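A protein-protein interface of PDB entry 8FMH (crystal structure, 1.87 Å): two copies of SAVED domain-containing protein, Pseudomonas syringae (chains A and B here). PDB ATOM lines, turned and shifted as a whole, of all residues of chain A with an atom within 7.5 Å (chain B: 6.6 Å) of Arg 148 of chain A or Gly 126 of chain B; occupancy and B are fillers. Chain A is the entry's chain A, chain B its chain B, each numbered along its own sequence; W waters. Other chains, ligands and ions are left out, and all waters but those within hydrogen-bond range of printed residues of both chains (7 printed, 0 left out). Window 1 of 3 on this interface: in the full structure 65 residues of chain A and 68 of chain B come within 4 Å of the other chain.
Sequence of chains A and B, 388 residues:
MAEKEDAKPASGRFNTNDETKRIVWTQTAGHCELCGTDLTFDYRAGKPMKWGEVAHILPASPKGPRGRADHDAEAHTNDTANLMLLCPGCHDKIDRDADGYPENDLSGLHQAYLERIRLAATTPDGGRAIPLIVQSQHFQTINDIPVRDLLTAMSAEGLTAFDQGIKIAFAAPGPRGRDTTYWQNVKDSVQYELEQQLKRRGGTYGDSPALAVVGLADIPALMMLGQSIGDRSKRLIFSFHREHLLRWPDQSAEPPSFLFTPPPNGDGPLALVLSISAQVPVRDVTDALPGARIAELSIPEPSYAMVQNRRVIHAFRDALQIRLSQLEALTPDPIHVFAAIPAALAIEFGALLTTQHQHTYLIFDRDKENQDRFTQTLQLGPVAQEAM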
ATOM      1  N   CYS A  35      21.833 -17.355  30.047  1.00  0.00           N
ATOM      2  CA  CYS A  35      21.121 -17.718  28.827  1.00  0.00           C
ATOM      3  C   CYS A  35      20.704 -16.521  27.979  1.00  0.00           C
ATOM      4  O   CYS A  35      20.171 -16.720  26.885  1.00  0.00           O
ATOM      5  CB  CYS A  35      19.875 -18.564  29.153  1.00  0.00           C
ATOM      6  SG  CYS A  35      18.487 -17.686  29.908  1.00  0.00           S
ATOM      7  N   GLY A  36      20.928 -15.296  28.442  1.00  0.00           N
ATOM      8  CA  GLY A  36      20.685 -14.128  27.625  1.00  0.00           C
ATOM      9  C   GLY A  36      19.243 -13.681  27.528  1.00  0.00           C
ATOM     10  O   GLY A  36      18.968 -12.694  26.831  1.00  0.00           O
ATOM     11  N   ILE A 133      26.383 -12.105   4.459  1.00  0.00           N
ATOM     12  CA  ILE A 133      27.072 -13.384   4.516  1.00  0.00           C
ATOM     13  C   ILE A 133      26.806 -14.112   3.210  1.00  0.00           C
ATOM     14  O   ILE A 133      25.652 -14.228   2.782  1.00  0.00           O
ATOM     15  CB  ILE A 133      26.609 -14.233   5.714  1.00  0.00           C
ATOM     16  CG1 ILE A 133      27.014 -13.558   7.024  1.00  0.00           C
ATOM     17  CG2 ILE A 133      27.188 -15.646   5.633  1.00  0.00           C
ATOM     18  CD1 ILE A 133      26.387 -14.187   8.254  1.00  0.00           C
ATOM     19  N   ILE A 145      28.441 -19.778   8.498  1.00  0.00           N
ATOM     20  CA  ILE A 145      28.943 -18.638   9.260  1.00  0.00           C
ATOM     21  C   ILE A 145      27.831 -18.170  10.191  1.00  0.00           C
ATOM     22  O   ILE A 145      26.728 -17.863   9.714  1.00  0.00           O
ATOM     23  CB  ILE A 145      29.402 -17.511   8.324  1.00  0.00           C
ATOM     24  CG1 ILE A 145      30.465 -18.044   7.361  1.00  0.00           C
ATOM     25  CG2 ILE A 145      29.931 -16.324   9.121  1.00  0.00           C
ATOM     26  CD1 ILE A 145      30.853 -17.068   6.280  1.00  0.00           C
ATOM     27  N   PRO A 146      28.052 -18.102  11.506  1.00  0.00           N
ATOM     28  CA  PRO A 146      26.984 -17.630  12.397  1.00  0.00           C
ATOM     29  C   PRO A 146      26.716 -16.147  12.191  1.00  0.00           C
ATOM     30  O   PRO A 146      27.643 -15.338  12.101  1.00  0.00           O
ATOM     31  CB  PRO A 146      27.529 -17.916  13.804  1.00  0.00           C
ATOM     32  CG  PRO A 146      28.693 -18.836  13.614  1.00  0.00           C
ATOM     33  CD  PRO A 146      29.247 -18.514  12.262  1.00  0.00           C
ATOM     34  N   VAL A 147      25.429 -15.797  12.113  1.00  0.00           N
ATOM     35  CA  VAL A 147      25.037 -14.397  11.976  1.00  0.00           C
ATOM     36  C   VAL A 147      25.536 -13.584  13.163  1.00  0.00           C
ATOM     37  O   VAL A 147      26.037 -12.465  12.999  1.00  0.00           O
ATOM     38  CB  VAL A 147      23.506 -14.297  11.821  1.00  0.00           C
ATOM     39  CG1 VAL A 147      23.027 -12.875  11.973  1.00  0.00           C
ATOM     40  CG2 VAL A 147      23.089 -14.827  10.470  1.00  0.00           C
ATOM     41  N   ARG A 148      25.405 -14.127  14.376  1.00  0.00           N
ATOM     42  CA  ARG A 148      25.789 -13.370  15.566  1.00  0.00           C
ATOM     43  C   ARG A 148      27.269 -13.023  15.549  1.00  0.00           C
ATOM     44  O   ARG A 148      27.668 -11.949  16.017  1.00  0.00           O
ATOM     45  CB  ARG A 148      25.449 -14.161  16.829  1.00  0.00           C
ATOM     46  CG  ARG A 148      25.976 -13.527  18.106  1.00  0.00           C
ATOM     47  CD  ARG A 148      25.602 -14.323  19.343  1.00  0.00           C
ATOM     48  NE  ARG A 148      24.195 -14.182  19.698  1.00  0.00           N
ATOM     49  CZ  ARG A 148      23.690 -13.152  20.360  1.00  0.00           C
ATOM     50  NH1 ARG A 148      24.439 -12.119  20.707  1.00  0.00           N
ATOM     51  NH2 ARG A 148      22.399 -13.155  20.679  1.00  0.00           N
ATOM     52  N   ASP A 149      28.103 -13.919  15.025  1.00  0.00           N
ATOM     53  CA  ASP A 149      29.537 -13.658  15.024  1.00  0.00           C
ATOM     54  C   ASP A 149      29.902 -12.505  14.093  1.00  0.00           C
ATOM     55  O   ASP A 149      30.840 -11.751  14.382  1.00  0.00           O
ATOM     56  CB  ASP A 149      30.290 -14.933  14.648  1.00  0.00           C
ATOM     57  CG  ASP A 149      30.292 -15.951  15.771  1.00  0.00           C
ATOM     58  OD1 ASP A 149      29.236 -16.556  16.030  1.00  0.00           O
ATOM     59  OD2 ASP A 149      31.346 -16.135  16.410  1.00  0.00           O
ATOM     60  N   LEU A 150      29.177 -12.342  12.982  1.00  0.00           N
ATOM     61  CA  LEU A 150      29.392 -11.176  12.132  1.00  0.00           C
ATOM     62  C   LEU A 150      28.946  -9.898  12.836  1.00  0.00           C
ATOM     63  O   LEU A 150      29.669  -8.895  12.840  1.00  0.00           O
ATOM     64  CB  LEU A 150      28.650 -11.346  10.806  1.00  0.00           C
ATOM     65  CG  LEU A 150      28.666 -10.120   9.888  1.00  0.00           C
ATOM     66  CD1 LEU A 150      30.095  -9.746   9.525  1.00  0.00           C
ATOM     67  CD2 LEU A 150      27.845 -10.354   8.634  1.00  0.00           C
ATOM     68  N   LEU A 151      27.752  -9.913  13.438  1.00  0.00           N
ATOM     69  CA  LEU A 151      27.260  -8.725  14.125  1.00  0.00           C
ATOM     70  C   LEU A 151      28.177  -8.340  15.277  1.00  0.00           C
ATOM     71  O   LEU A 151      28.417  -7.151  15.523  1.00  0.00           O
ATOM     72  CB  LEU A 151      25.839  -8.964  14.629  1.00  0.00           C
ATOM     73  CG  LEU A 151      24.809  -9.281  13.544  1.00  0.00           C
ATOM     74  CD1 LEU A 151      23.460  -9.607  14.168  1.00  0.00           C
ATOM     75  CD2 LEU A 151      24.688  -8.123  12.564  1.00  0.00           C
ATOM     76  N   THR A 152      28.697  -9.336  15.995  1.00  0.00           N
ATOM     77  CA  THR A 152      29.634  -9.064  17.081  1.00  0.00           C
ATOM     78  C   THR A 152      30.943  -8.497  16.547  1.00  0.00           C
ATOM     79  O   THR A 152      31.545  -7.615  17.171  1.00  0.00           O
ATOM     80  CB  THR A 152      29.876 -10.350  17.876  1.00  0.00           C
ATOM     81  OG1 THR A 152      28.650 -10.767  18.496  1.00  0.00           O
ATOM     82  CG2 THR A 152      30.924 -10.141  18.948  1.00  0.00           C
ATOM     83  N   ALA A 153      31.411  -9.004  15.406  1.00  0.00           N
ATOM     84  CA  ALA A 153      32.592  -8.428  14.775  1.00  0.00           C
ATOM     85  C   ALA A 153      32.328  -6.994  14.343  1.00  0.00           C
ATOM     86  O   ALA A 153      33.190  -6.121  14.494  1.00  0.00           O
ATOM     87  CB  ALA A 153      33.011  -9.278  13.574  1.00  0.00           C
ATOM     88  N   MET A 154      31.141  -6.736  13.791  1.00  0.00           N
ATOM     89  CA  MET A 154      30.770  -5.374  13.429  1.00  0.00           C
ATOM     90  C   MET A 154      30.699  -4.486  14.659  1.00  0.00           C
ATOM     91  O   MET A 154      31.336  -3.428  14.712  1.00  0.00           O
ATOM     92  CB  MET A 154      29.429  -5.378  12.698  1.00  0.00           C
ATOM     93  CG  MET A 154      29.468  -6.067  11.343  1.00  0.00           C
ATOM     94  SD  MET A 154      27.830  -6.273  10.630  1.00  0.00           S
ATOM     95  CE  MET A 154      27.254  -4.575  10.621  1.00  0.00           C
ATOM     96  N   SER A 155      29.926  -4.902  15.666  1.00  0.00           N
ATOM     97  CA  SER A 155      29.797  -4.093  16.873  1.00  0.00           C
ATOM     98  C   SER A 155      31.159  -3.743  17.453  1.00  0.00           C
ATOM     99  O   SER A 155      31.360  -2.636  17.966  1.00  0.00           O
ATOM    100  CB  SER A 155      28.957  -4.829  17.918  1.00  0.00           C
ATOM    101  OG  SER A 155      28.914  -4.073  19.124  1.00  0.00           O
ATOM    102  N   GLN A 164      19.301  -8.091  10.864  1.00  0.00           N
ATOM    103  CA  GLN A 164      20.427  -9.014  10.921  1.00  0.00           C
ATOM    104  C   GLN A 164      21.089  -9.213   9.567  1.00  0.00           C
ATOM    105  O   GLN A 164      22.080  -9.953   9.485  1.00  0.00           O
ATOM    106  CB  GLN A 164      19.989 -10.360  11.493  1.00  0.00           C
ATOM    107  CG  GLN A 164      19.191 -11.237  10.562  1.00  0.00           C
ATOM    108  CD  GLN A 164      18.888 -12.574  11.193  1.00  0.00           C
ATOM    109  OE1 GLN A 164      19.417 -13.605  10.777  1.00  0.00           O
ATOM    110  NE2 GLN A 164      18.041 -12.564  12.216  1.00  0.00           N
ATOM    111  N   LYS A 167      21.862 -13.164   4.190  1.00  0.00           N
ATOM    112  CA  LYS A 167      22.632 -14.401   4.272  1.00  0.00           C
ATOM    113  C   LYS A 167      22.261 -15.257   3.072  1.00  0.00           C
ATOM    114  O   LYS A 167      21.131 -15.745   2.974  1.00  0.00           O
ATOM    115  CB  LYS A 167      22.374 -15.145   5.580  1.00  0.00           C
ATOM    116  CG  LYS A 167      23.224 -16.399   5.732  1.00  0.00           C
ATOM    117  CD  LYS A 167      23.292 -16.867   7.175  1.00  0.00           C
ATOM    118  CE  LYS A 167      24.126 -18.121   7.312  1.00  0.00           C
ATOM    119  NZ  LYS A 167      24.231 -18.563   8.728  1.00  0.00           N
ATOM    120  N   LEU A 245      37.350 -17.528  14.262  1.00  0.00           N
ATOM    121  CA  LEU A 245      36.005 -17.353  13.713  1.00  0.00           C
ATOM    122  C   LEU A 245      35.950 -15.966  13.084  1.00  0.00           C
ATOM    123  O   LEU A 245      36.788 -15.677  12.213  1.00  0.00           O
ATOM    124  CB  LEU A 245      35.000 -17.642  14.830  1.00  0.00           C
ATOM    125  CG  LEU A 245      33.708 -18.315  14.361  1.00  0.00           C
ATOM    126  CD1 LEU A 245      32.899 -18.835  15.547  1.00  0.00           C
ATOM    127  CD2 LEU A 245      32.880 -17.348  13.512  1.00  0.00           C
ATOM    128  N   LEU A 246      35.021 -15.094  13.463  1.00  0.00           N
ATOM    129  CA  LEU A 246      34.945 -13.749  12.898  1.00  0.00           C
ATOM    130  C   LEU A 246      35.793 -12.732  13.646  1.00  0.00           C
ATOM    131  O   LEU A 246      35.826 -11.566  13.248  1.00  0.00           O
ATOM    132  CB  LEU A 246      33.492 -13.262  12.871  1.00  0.00           C
ATOM    133  CG  LEU A 246      32.780 -13.361  11.522  1.00  0.00           C
ATOM    134  CD1 LEU A 246      33.375 -12.357  10.535  1.00  0.00           C
ATOM    135  CD2 LEU A 246      32.868 -14.769  10.969  1.00  0.00           C
ATOM    136  N   ARG B 118      22.286  -4.586  23.467  1.00  0.00           N
ATOM    137  CA  ARG B 118      21.461  -5.780  23.305  1.00  0.00           C
ATOM    138  C   ARG B 118      22.285  -6.956  22.804  1.00  0.00           C
ATOM    139  O   ARG B 118      22.143  -8.077  23.303  1.00  0.00           O
ATOM    140  CB  ARG B 118      20.301  -5.498  22.348  1.00  0.00           C
ATOM    141  N   LEU B 119      23.153  -6.721  21.815  1.00  0.00           N
ATOM    142  CA  LEU B 119      23.963  -7.807  21.266  1.00  0.00           C
ATOM    143  C   LEU B 119      24.864  -8.416  22.334  1.00  0.00           C
ATOM    144  O   LEU B 119      25.067  -9.634  22.365  1.00  0.00           O
ATOM    145  CB  LEU B 119      24.793  -7.289  20.091  1.00  0.00           C
ATOM    146  CG  LEU B 119      25.719  -8.287  19.399  1.00  0.00           C
ATOM    147  CD1 LEU B 119      24.924  -9.339  18.665  1.00  0.00           C
ATOM    148  CD2 LEU B 119      26.631  -7.571  18.432  1.00  0.00           C
ATOM    149  N   ALA B 120      25.424  -7.581  23.210  1.00  0.00           N
ATOM    150  CA  ALA B 120      26.245  -8.096  24.301  1.00  0.00           C
ATOM    151  C   ALA B 120      25.396  -8.815  25.342  1.00  0.00           C
ATOM    152  O   ALA B 120      25.759  -9.901  25.809  1.00  0.00           O
ATOM    153  CB  ALA B 120      27.026  -6.951  24.948  1.00  0.00           C
ATOM    154  N   ALA B 121      24.258  -8.227  25.714  1.00  0.00           N
ATOM    155  CA  ALA B 121      23.422  -8.819  26.752  1.00  0.00           C
ATOM    156  C   ALA B 121      22.871 -10.178  26.337  1.00  0.00           C
ATOM    157  O   ALA B 121      22.642 -11.037  27.193  1.00  0.00           O
ATOM    158  CB  ALA B 121      22.281  -7.866  27.095  1.00  0.00           C
ATOM    159  N   THR B 122      22.653 -10.397  25.042  1.00  0.00           N
ATOM    160  CA  THR B 122      22.128 -11.663  24.549  1.00  0.00           C
ATOM    161  C   THR B 122      23.216 -12.634  24.121  1.00  0.00           C
ATOM    162  O   THR B 122      22.891 -13.723  23.645  1.00  0.00           O
ATOM    163  CB  THR B 122      21.186 -11.430  23.363  1.00  0.00           C
ATOM    164  OG1 THR B 122      21.908 -10.825  22.282  1.00  0.00           O
ATOM    165  CG2 THR B 122      20.038 -10.532  23.766  1.00  0.00           C
ATOM    166  N   THR B 123      24.492 -12.274  24.272  1.00  0.00           N
ATOM    167  CA  THR B 123      25.567 -13.160  23.831  1.00  0.00           C
ATOM    168  C   THR B 123      25.481 -14.553  24.444  1.00  0.00           C
ATOM    169  O   THR B 123      25.840 -15.525  23.754  1.00  0.00           O
ATOM    170  CB  THR B 123      26.924 -12.518  24.147  1.00  0.00           C
ATOM    171  OG1 THR B 123      27.023 -11.255  23.479  1.00  0.00           O
ATOM    172  CG2 THR B 123      28.067 -13.414  23.688  1.00  0.00           C
ATOM    173  N   PRO B 124      25.031 -14.731  25.687  1.00  0.00           N
ATOM    174  CA  PRO B 124      24.936 -16.095  26.231  1.00  0.00           C
ATOM    175  C   PRO B 124      24.149 -17.058  25.354  1.00  0.00           C
ATOM    176  O   PRO B 124      24.470 -18.255  25.343  1.00  0.00           O
ATOM    177  CB  PRO B 124      24.269 -15.875  27.594  1.00  0.00           C
ATOM    178  CG  PRO B 124      24.695 -14.502  27.988  1.00  0.00           C
ATOM    179  CD  PRO B 124      24.745 -13.710  26.713  1.00  0.00           C
ATOM    180  N   ASP B 125      23.142 -16.595  24.607  1.00  0.00           N
ATOM    181  CA  ASP B 125      22.430 -17.507  23.714  1.00  0.00           C
ATOM    182  C   ASP B 125      23.237 -17.852  22.471  1.00  0.00           C
ATOM    183  O   ASP B 125      22.810 -18.712  21.695  1.00  0.00           O
ATOM    184  CB  ASP B 125      21.065 -16.931  23.301  1.00  0.00           C
ATOM    185  CG  ASP B 125      21.134 -16.037  22.062  1.00  0.00           C
ATOM    186  OD1 ASP B 125      21.569 -16.504  20.989  1.00  0.00           O
ATOM    187  OD2 ASP B 125      20.713 -14.863  22.154  1.00  0.00           O
ATOM    188  N   GLY B 126      24.375 -17.201  22.250  1.00  0.00           N
ATOM    189  CA  GLY B 126      25.261 -17.632  21.192  1.00  0.00           C
ATOM    190  C   GLY B 126      25.998 -18.919  21.486  1.00  0.00           C
ATOM    191  O   GLY B 126      26.782 -19.379  20.648  1.00  0.00           O
ATOM    192  N   GLY B 127      25.758 -19.508  22.658  1.00  0.00           N
ATOM    193  CA  GLY B 127      26.407 -20.724  23.090  1.00  0.00           C
ATOM    194  C   GLY B 127      25.589 -21.986  22.945  1.00  0.00           C
ATOM    195  O   GLY B 127      26.094 -23.062  23.282  1.00  0.00           O
ATOM    196  N   ARG B 128      24.336 -21.896  22.488  1.00  0.00           N
ATOM    197  CA  ARG B 128      23.566 -23.089  22.159  1.00  0.00           C
ATOM    198  C   ARG B 128      24.457 -24.083  21.437  1.00  0.00           C
ATOM    199  O   ARG B 128      25.155 -23.726  20.485  1.00  0.00           O
ATOM    200  CB  ARG B 128      22.365 -22.733  21.280  1.00  0.00           C
ATOM    201  CG  ARG B 128      21.276 -21.965  21.992  1.00  0.00           C
ATOM    202  CD  ARG B 128      20.064 -21.721  21.096  1.00  0.00           C
ATOM    203  NE  ARG B 128      19.210 -22.897  20.956  1.00  0.00           N
ATOM    204  CZ  ARG B 128      19.145 -23.672  19.879  1.00  0.00           C
ATOM    205  NH1 ARG B 128      19.895 -23.447  18.811  1.00  0.00           N
ATOM    206  NH2 ARG B 128      18.301 -24.702  19.874  1.00  0.00           N
ATOM    207  N   ALA B 129      24.446 -25.331  21.902  1.00  0.00           N
ATOM    208  CA  ALA B 129      25.435 -26.284  21.428  1.00  0.00           C
ATOM    209  C   ALA B 129      24.879 -27.696  21.447  1.00  0.00           C
ATOM    210  O   ALA B 129      23.921 -28.011  22.161  1.00  0.00           O
ATOM    211  CB  ALA B 129      26.708 -26.225  22.274  1.00  0.00           C
ATOM    212  N   GLY B 158      30.767 -21.541  28.383  1.00  0.00           N
ATOM    213  CA  GLY B 158      29.605 -20.864  27.847  1.00  0.00           C
ATOM    214  C   GLY B 158      28.830 -21.622  26.788  1.00  0.00           C
ATOM    215  O   GLY B 158      27.918 -21.044  26.183  1.00  0.00           O
ATOM    216  N   LEU B 159      29.161 -22.886  26.538  1.00  0.00           N
ATOM    217  CA  LEU B 159      28.406 -23.723  25.613  1.00  0.00           C
ATOM    218  C   LEU B 159      27.299 -24.450  26.366  1.00  0.00           C
ATOM    219  O   LEU B 159      27.566 -25.144  27.352  1.00  0.00           O
ATOM    220  CB  LEU B 159      29.327 -24.732  24.936  1.00  0.00           C
ATOM    221  CG  LEU B 159      30.439 -24.179  24.052  1.00  0.00           C
ATOM    222  CD1 LEU B 159      31.336 -25.320  23.605  1.00  0.00           C
ATOM    223  CD2 LEU B 159      29.872 -23.438  22.847  1.00  0.00           C
ATOM    224  N   THR B 160      26.060 -24.301  25.892  1.00  0.00           N
ATOM    225  CA  THR B 160      24.875 -24.772  26.607  1.00  0.00           C
ATOM    226  C   THR B 160      24.074 -25.722  25.724  1.00  0.00           C
ATOM    227  O   THR B 160      23.422 -25.287  24.768  1.00  0.00           O
ATOM    228  CB  THR B 160      23.999 -23.597  27.024  1.00  0.00           C
ATOM    229  OG1 THR B 160      23.436 -23.002  25.849  1.00  0.00           O
ATOM    230  CG2 THR B 160      24.813 -22.552  27.771  1.00  0.00           C
ATOM    231  N   GLY B 203      18.154 -19.175  19.315  1.00  0.00           N
ATOM    232  CA  GLY B 203      18.822 -17.963  19.725  1.00  0.00           C
ATOM    233  C   GLY B 203      18.182 -16.739  19.095  1.00  0.00           C
ATOM    234  O   GLY B 203      17.068 -16.774  18.561  1.00  0.00           O
ATOM    235  N   THR B 204      18.926 -15.636  19.141  1.00  0.00           N
ATOM    236  CA  THR B 204      18.372 -14.352  18.733  1.00  0.00           C
ATOM    237  C   THR B 204      18.259 -14.205  17.221  1.00  0.00           C
ATOM    238  O   THR B 204      17.401 -13.453  16.749  1.00  0.00           O
ATOM    239  CB  THR B 204      19.234 -13.223  19.291  1.00  0.00           C
ATOM    240  OG1 THR B 204      19.407 -13.414  20.703  1.00  0.00           O
ATOM    241  CG2 THR B 204      18.573 -11.870  19.031  1.00  0.00           C
ATOM    242  N   TYR B 205      19.102 -14.896  16.449  1.00  0.00           N
ATOM    243  CA  TYR B 205      19.187 -14.683  15.010  1.00  0.00           C
ATOM    244  C   TYR B 205      18.930 -15.948  14.204  1.00  0.00           C
ATOM    245  O   TYR B 205      19.209 -15.965  13.000  1.00  0.00           O
ATOM    246  CB  TYR B 205      20.560 -14.111  14.642  1.00  0.00           C
ATOM    247  CG  TYR B 205      20.924 -12.866  15.413  1.00  0.00           C
ATOM    248  CD1 TYR B 205      20.316 -11.649  15.138  1.00  0.00           C
ATOM    249  CD2 TYR B 205      21.877 -12.906  16.416  1.00  0.00           C
ATOM    250  CE1 TYR B 205      20.648 -10.511  15.844  1.00  0.00           C
ATOM    251  CE2 TYR B 205      22.216 -11.772  17.126  1.00  0.00           C
ATOM    252  CZ  TYR B 205      21.600 -10.582  16.833  1.00  0.00           C
ATOM    253  OH  TYR B 205      21.936  -9.457  17.549  1.00  0.00           O
ATOM    254  N   ASP B 207      20.521 -18.725  14.312  1.00  0.00           N
ATOM    255  CA  ASP B 207      21.756 -19.431  14.000  1.00  0.00           C
ATOM    256  C   ASP B 207      21.649 -20.906  14.360  1.00  0.00           C
ATOM    257  O   ASP B 207      20.965 -21.291  15.312  1.00  0.00           O
ATOM    258  CB  ASP B 207      22.934 -18.827  14.769  1.00  0.00           C
ATOM    259  CG  ASP B 207      23.513 -17.602  14.101  1.00  0.00           C
ATOM    260  OD1 ASP B 207      23.395 -17.479  12.863  1.00  0.00           O
ATOM    261  OD2 ASP B 207      24.105 -16.769  14.817  1.00  0.00           O
ATOM    262  N   SER B 208      22.352 -21.734  13.593  1.00  0.00           N
ATOM    263  CA  SER B 208      22.531 -23.119  13.985  1.00  0.00           C
ATOM    264  C   SER B 208      23.366 -23.199  15.261  1.00  0.00           C
ATOM    265  O   SER B 208      24.213 -22.338  15.519  1.00  0.00           O
ATOM    266  CB  SER B 208      23.214 -23.915  12.877  1.00  0.00           C
ATOM    267  OG  SER B 208      22.279 -24.310  11.893  1.00  0.00           O
ATOM    268  N   ALA B 210      26.231 -24.523  17.989  1.00  0.00           N
ATOM    269  CA  ALA B 210      27.624 -24.922  17.897  1.00  0.00           C
ATOM    270  C   ALA B 210      27.763 -26.418  18.134  1.00  0.00           C
ATOM    271  O   ALA B 210      26.969 -27.030  18.847  1.00  0.00           O
ATOM    272  CB  ALA B 210      28.464 -24.157  18.918  1.00  0.00           C
ATOM    273  N   LYS B 234      30.721 -23.129  13.447  1.00  0.00           N
ATOM    274  CA  LYS B 234      31.008 -22.923  14.865  1.00  0.00           C
ATOM    275  C   LYS B 234      31.122 -24.290  15.521  1.00  0.00           C
ATOM    276  O   LYS B 234      30.117 -24.931  15.829  1.00  0.00           O
ATOM    277  CB  LYS B 234      29.938 -22.078  15.542  1.00  0.00           C
ATOM    278  CG  LYS B 234      30.297 -21.749  16.982  1.00  0.00           C
ATOM    279  CD  LYS B 234      29.408 -20.679  17.584  1.00  0.00           C
ATOM    280  CE  LYS B 234      29.659 -20.568  19.078  1.00  0.00           C
ATOM    281  NZ  LYS B 234      29.345 -19.220  19.629  1.00  0.00           N
HETATM  282  O   HOH W   1      24.099 -20.355  11.423  1.00  0.00           O
HETATM  283  O   HOH W   2      31.556 -17.306  19.214  1.00  0.00           O
HETATM  284  O   HOH W   3      27.902 -17.425  18.097  1.00  0.00           O
HETATM  285  O   HOH W   4      19.945 -16.991  10.516  1.00  0.00           O
HETATM  286  O   HOH W   5      22.976 -16.601  18.664  1.00  0.00           O
HETATM  287  O   HOH W   6      27.402 -11.748  20.694  1.00  0.00           O
HETATM  288  O   HOH W   7      22.235 -18.339  10.606  1.00  0.00           O
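O of Tyr 205 of chain B lies close to OE1 of Gln 164 of chain A (3.2 Å). N of Arg 148 of chain A lies within hydrogen-bond range of OD2 of Asp 207 of chain B, at 3.0 Å. OG1 of Thr 122 of chain B lies within hydrogen-bond range of NH2 of Arg 148 of chain A, at 2.9 Å. The guanidinium group (NH2) of Arg 148 of chain A is in salt-bridge range of the side-chain carboxylate (OD2) of Asp 125 of chain B (2.8 Å). NH1 of Arg 148 of chain A is in hydrogen-bond range of O of Leu 119 of chain B (3.1 Å). The side-chain hydroxyl (OG1) of Thr 204 of chain B lies within hydrogen-bond range of the guanidinium group (NH2) of Arg 148 of chain A, 3.0 Å away. OD1 of Asp 207 of chain B lies within hydrogen-bond range of N of Val 147 of chain A (2.7 Å).
O of Arg 118 of chain B sits at hydrogen-bond distance from OG1 of Thr 122 of chain B (2.9 Å). The side-chain hydroxyl (OG1) of Thr 123 of chain B lies within hydrogen-bond range of the backbone carbonyl oxygen (O) of Leu 119 of chain B, at 2.8 Å. OG1 of Thr 204 of chain B sits at hydrogen-bond distance from OD2 of Asp 125 of chain B, 2.4 Å away. O of Leu 119 of chain B is in hydrogen-bond range of OG1 of Thr 122 of chain B, at 3.4 Å. The backbone carbonyl oxygen (O) of Arg 148 of chain A is in hydrogen-bond range of the side-chain hydroxyl (OG1) of Thr 152 of chain A (2.9 Å). O of Ala 120 of chain B is in hydrogen-bond range of OG1 of Thr 123 of chain B (3.0 Å).
Among the printed residues, pairs that only touch across the chains: Leu 151 of chain A with Tyr 205 of chain B (3.4 Å), Leu 151 of chain A with Leu 119 of chain B (3.4 Å), Arg 148 of chain A with Thr 123 of chain B (3.5 Å), Gly 36 of chain A with Pro 124 of chain B (3.5 Å), Thr 152 of chain A with Leu 119 of chain B (3.6 Å), Pro 146 of chain A with Asp 207 of chain B (3.6 Å), Ser 155 of chain A with Leu 119 of chain B (3.6 Å), Cys 35 of chain A with Pro 124 of chain B (3.6 Å), Gly 36 of chain A with Ala 121 of chain B (3.7 Å), Cys 35 of chain A with Asp 125 of chain B (3.7 Å), Arg 148 of chain A with Gly 126 of chain B (3.8 Å), Arg 148 of chain A with Tyr 205 of chain B (3.8 Å), Val 147 of chain A with Tyr 205 of chain B (3.8 Å), Gly 36 of chain A with Thr 122 of chain B (3.9 Å) and Pro 146 of chain A with Lys 234 of chain B (3.97 Å).
Arg 148 of chain A touches just these residues of chain B: Leu 119 (3.1 Å), Thr 122 (2.9 Å), Thr 123 (3.5 Å), Asp 125 (2.8 Å), Gly 126 (3.8 Å), Thr 204 (3.0 Å), Tyr 205 (3.8 Å) and Asp 207 (3.0 Å). Gly 126 of chain B touches just one residue of chain A: Arg 148 (3.8 Å). Of the printed residues of chain B, Val 147 of chain A touches Tyr 205 and Asp 207. Printed residues of chain B within 4 Å of Ser 155 of chain A: Leu 119. The nearest printed residue of chain B that does not touch Thr 152 of chain A is Thr 123 of chain B (5.3 Å).
Of the 18 printed residues of chain A, 9 touch a printed residue of chain B. Among the printed residues, 22 pairs touch across the chains.
No position is printed for both chains.
Water W3 lies within hydrogen-bond range of the side-chain carboxylate (OD1) of Asp 149 of chain A (2.6 Å), the side-chain amino group (NZ) of Lys 234 of chain B (2.8 Å) and the backbone carbonyl oxygen (O) of Gly 126 of chain B (3.4 Å). Water W7 lies within hydrogen-bond range of OD1 of Asp 207 of chain B (2.7 Å) and NZ of Lys 167 of chain A (2.7 Å). Water W6 lies within hydrogen-bond range of the side-chain hydroxyl of Thr 152 of chain A (2.7 Å), the side-chain hydroxyl of Thr 123 of chain B (2.9 Å) and the guanidinium group of Arg 148 of chain A (3.0 Å). Water W5 bridges OD1 of Asp 125 of chain B (2.7 Å) and NE of Arg 148 of chain A (2.9 Å). Water W4 bridges O of Tyr 205 of chain B (2.8 Å) and OE1 of Gln 164 of chain A (3.4 Å).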
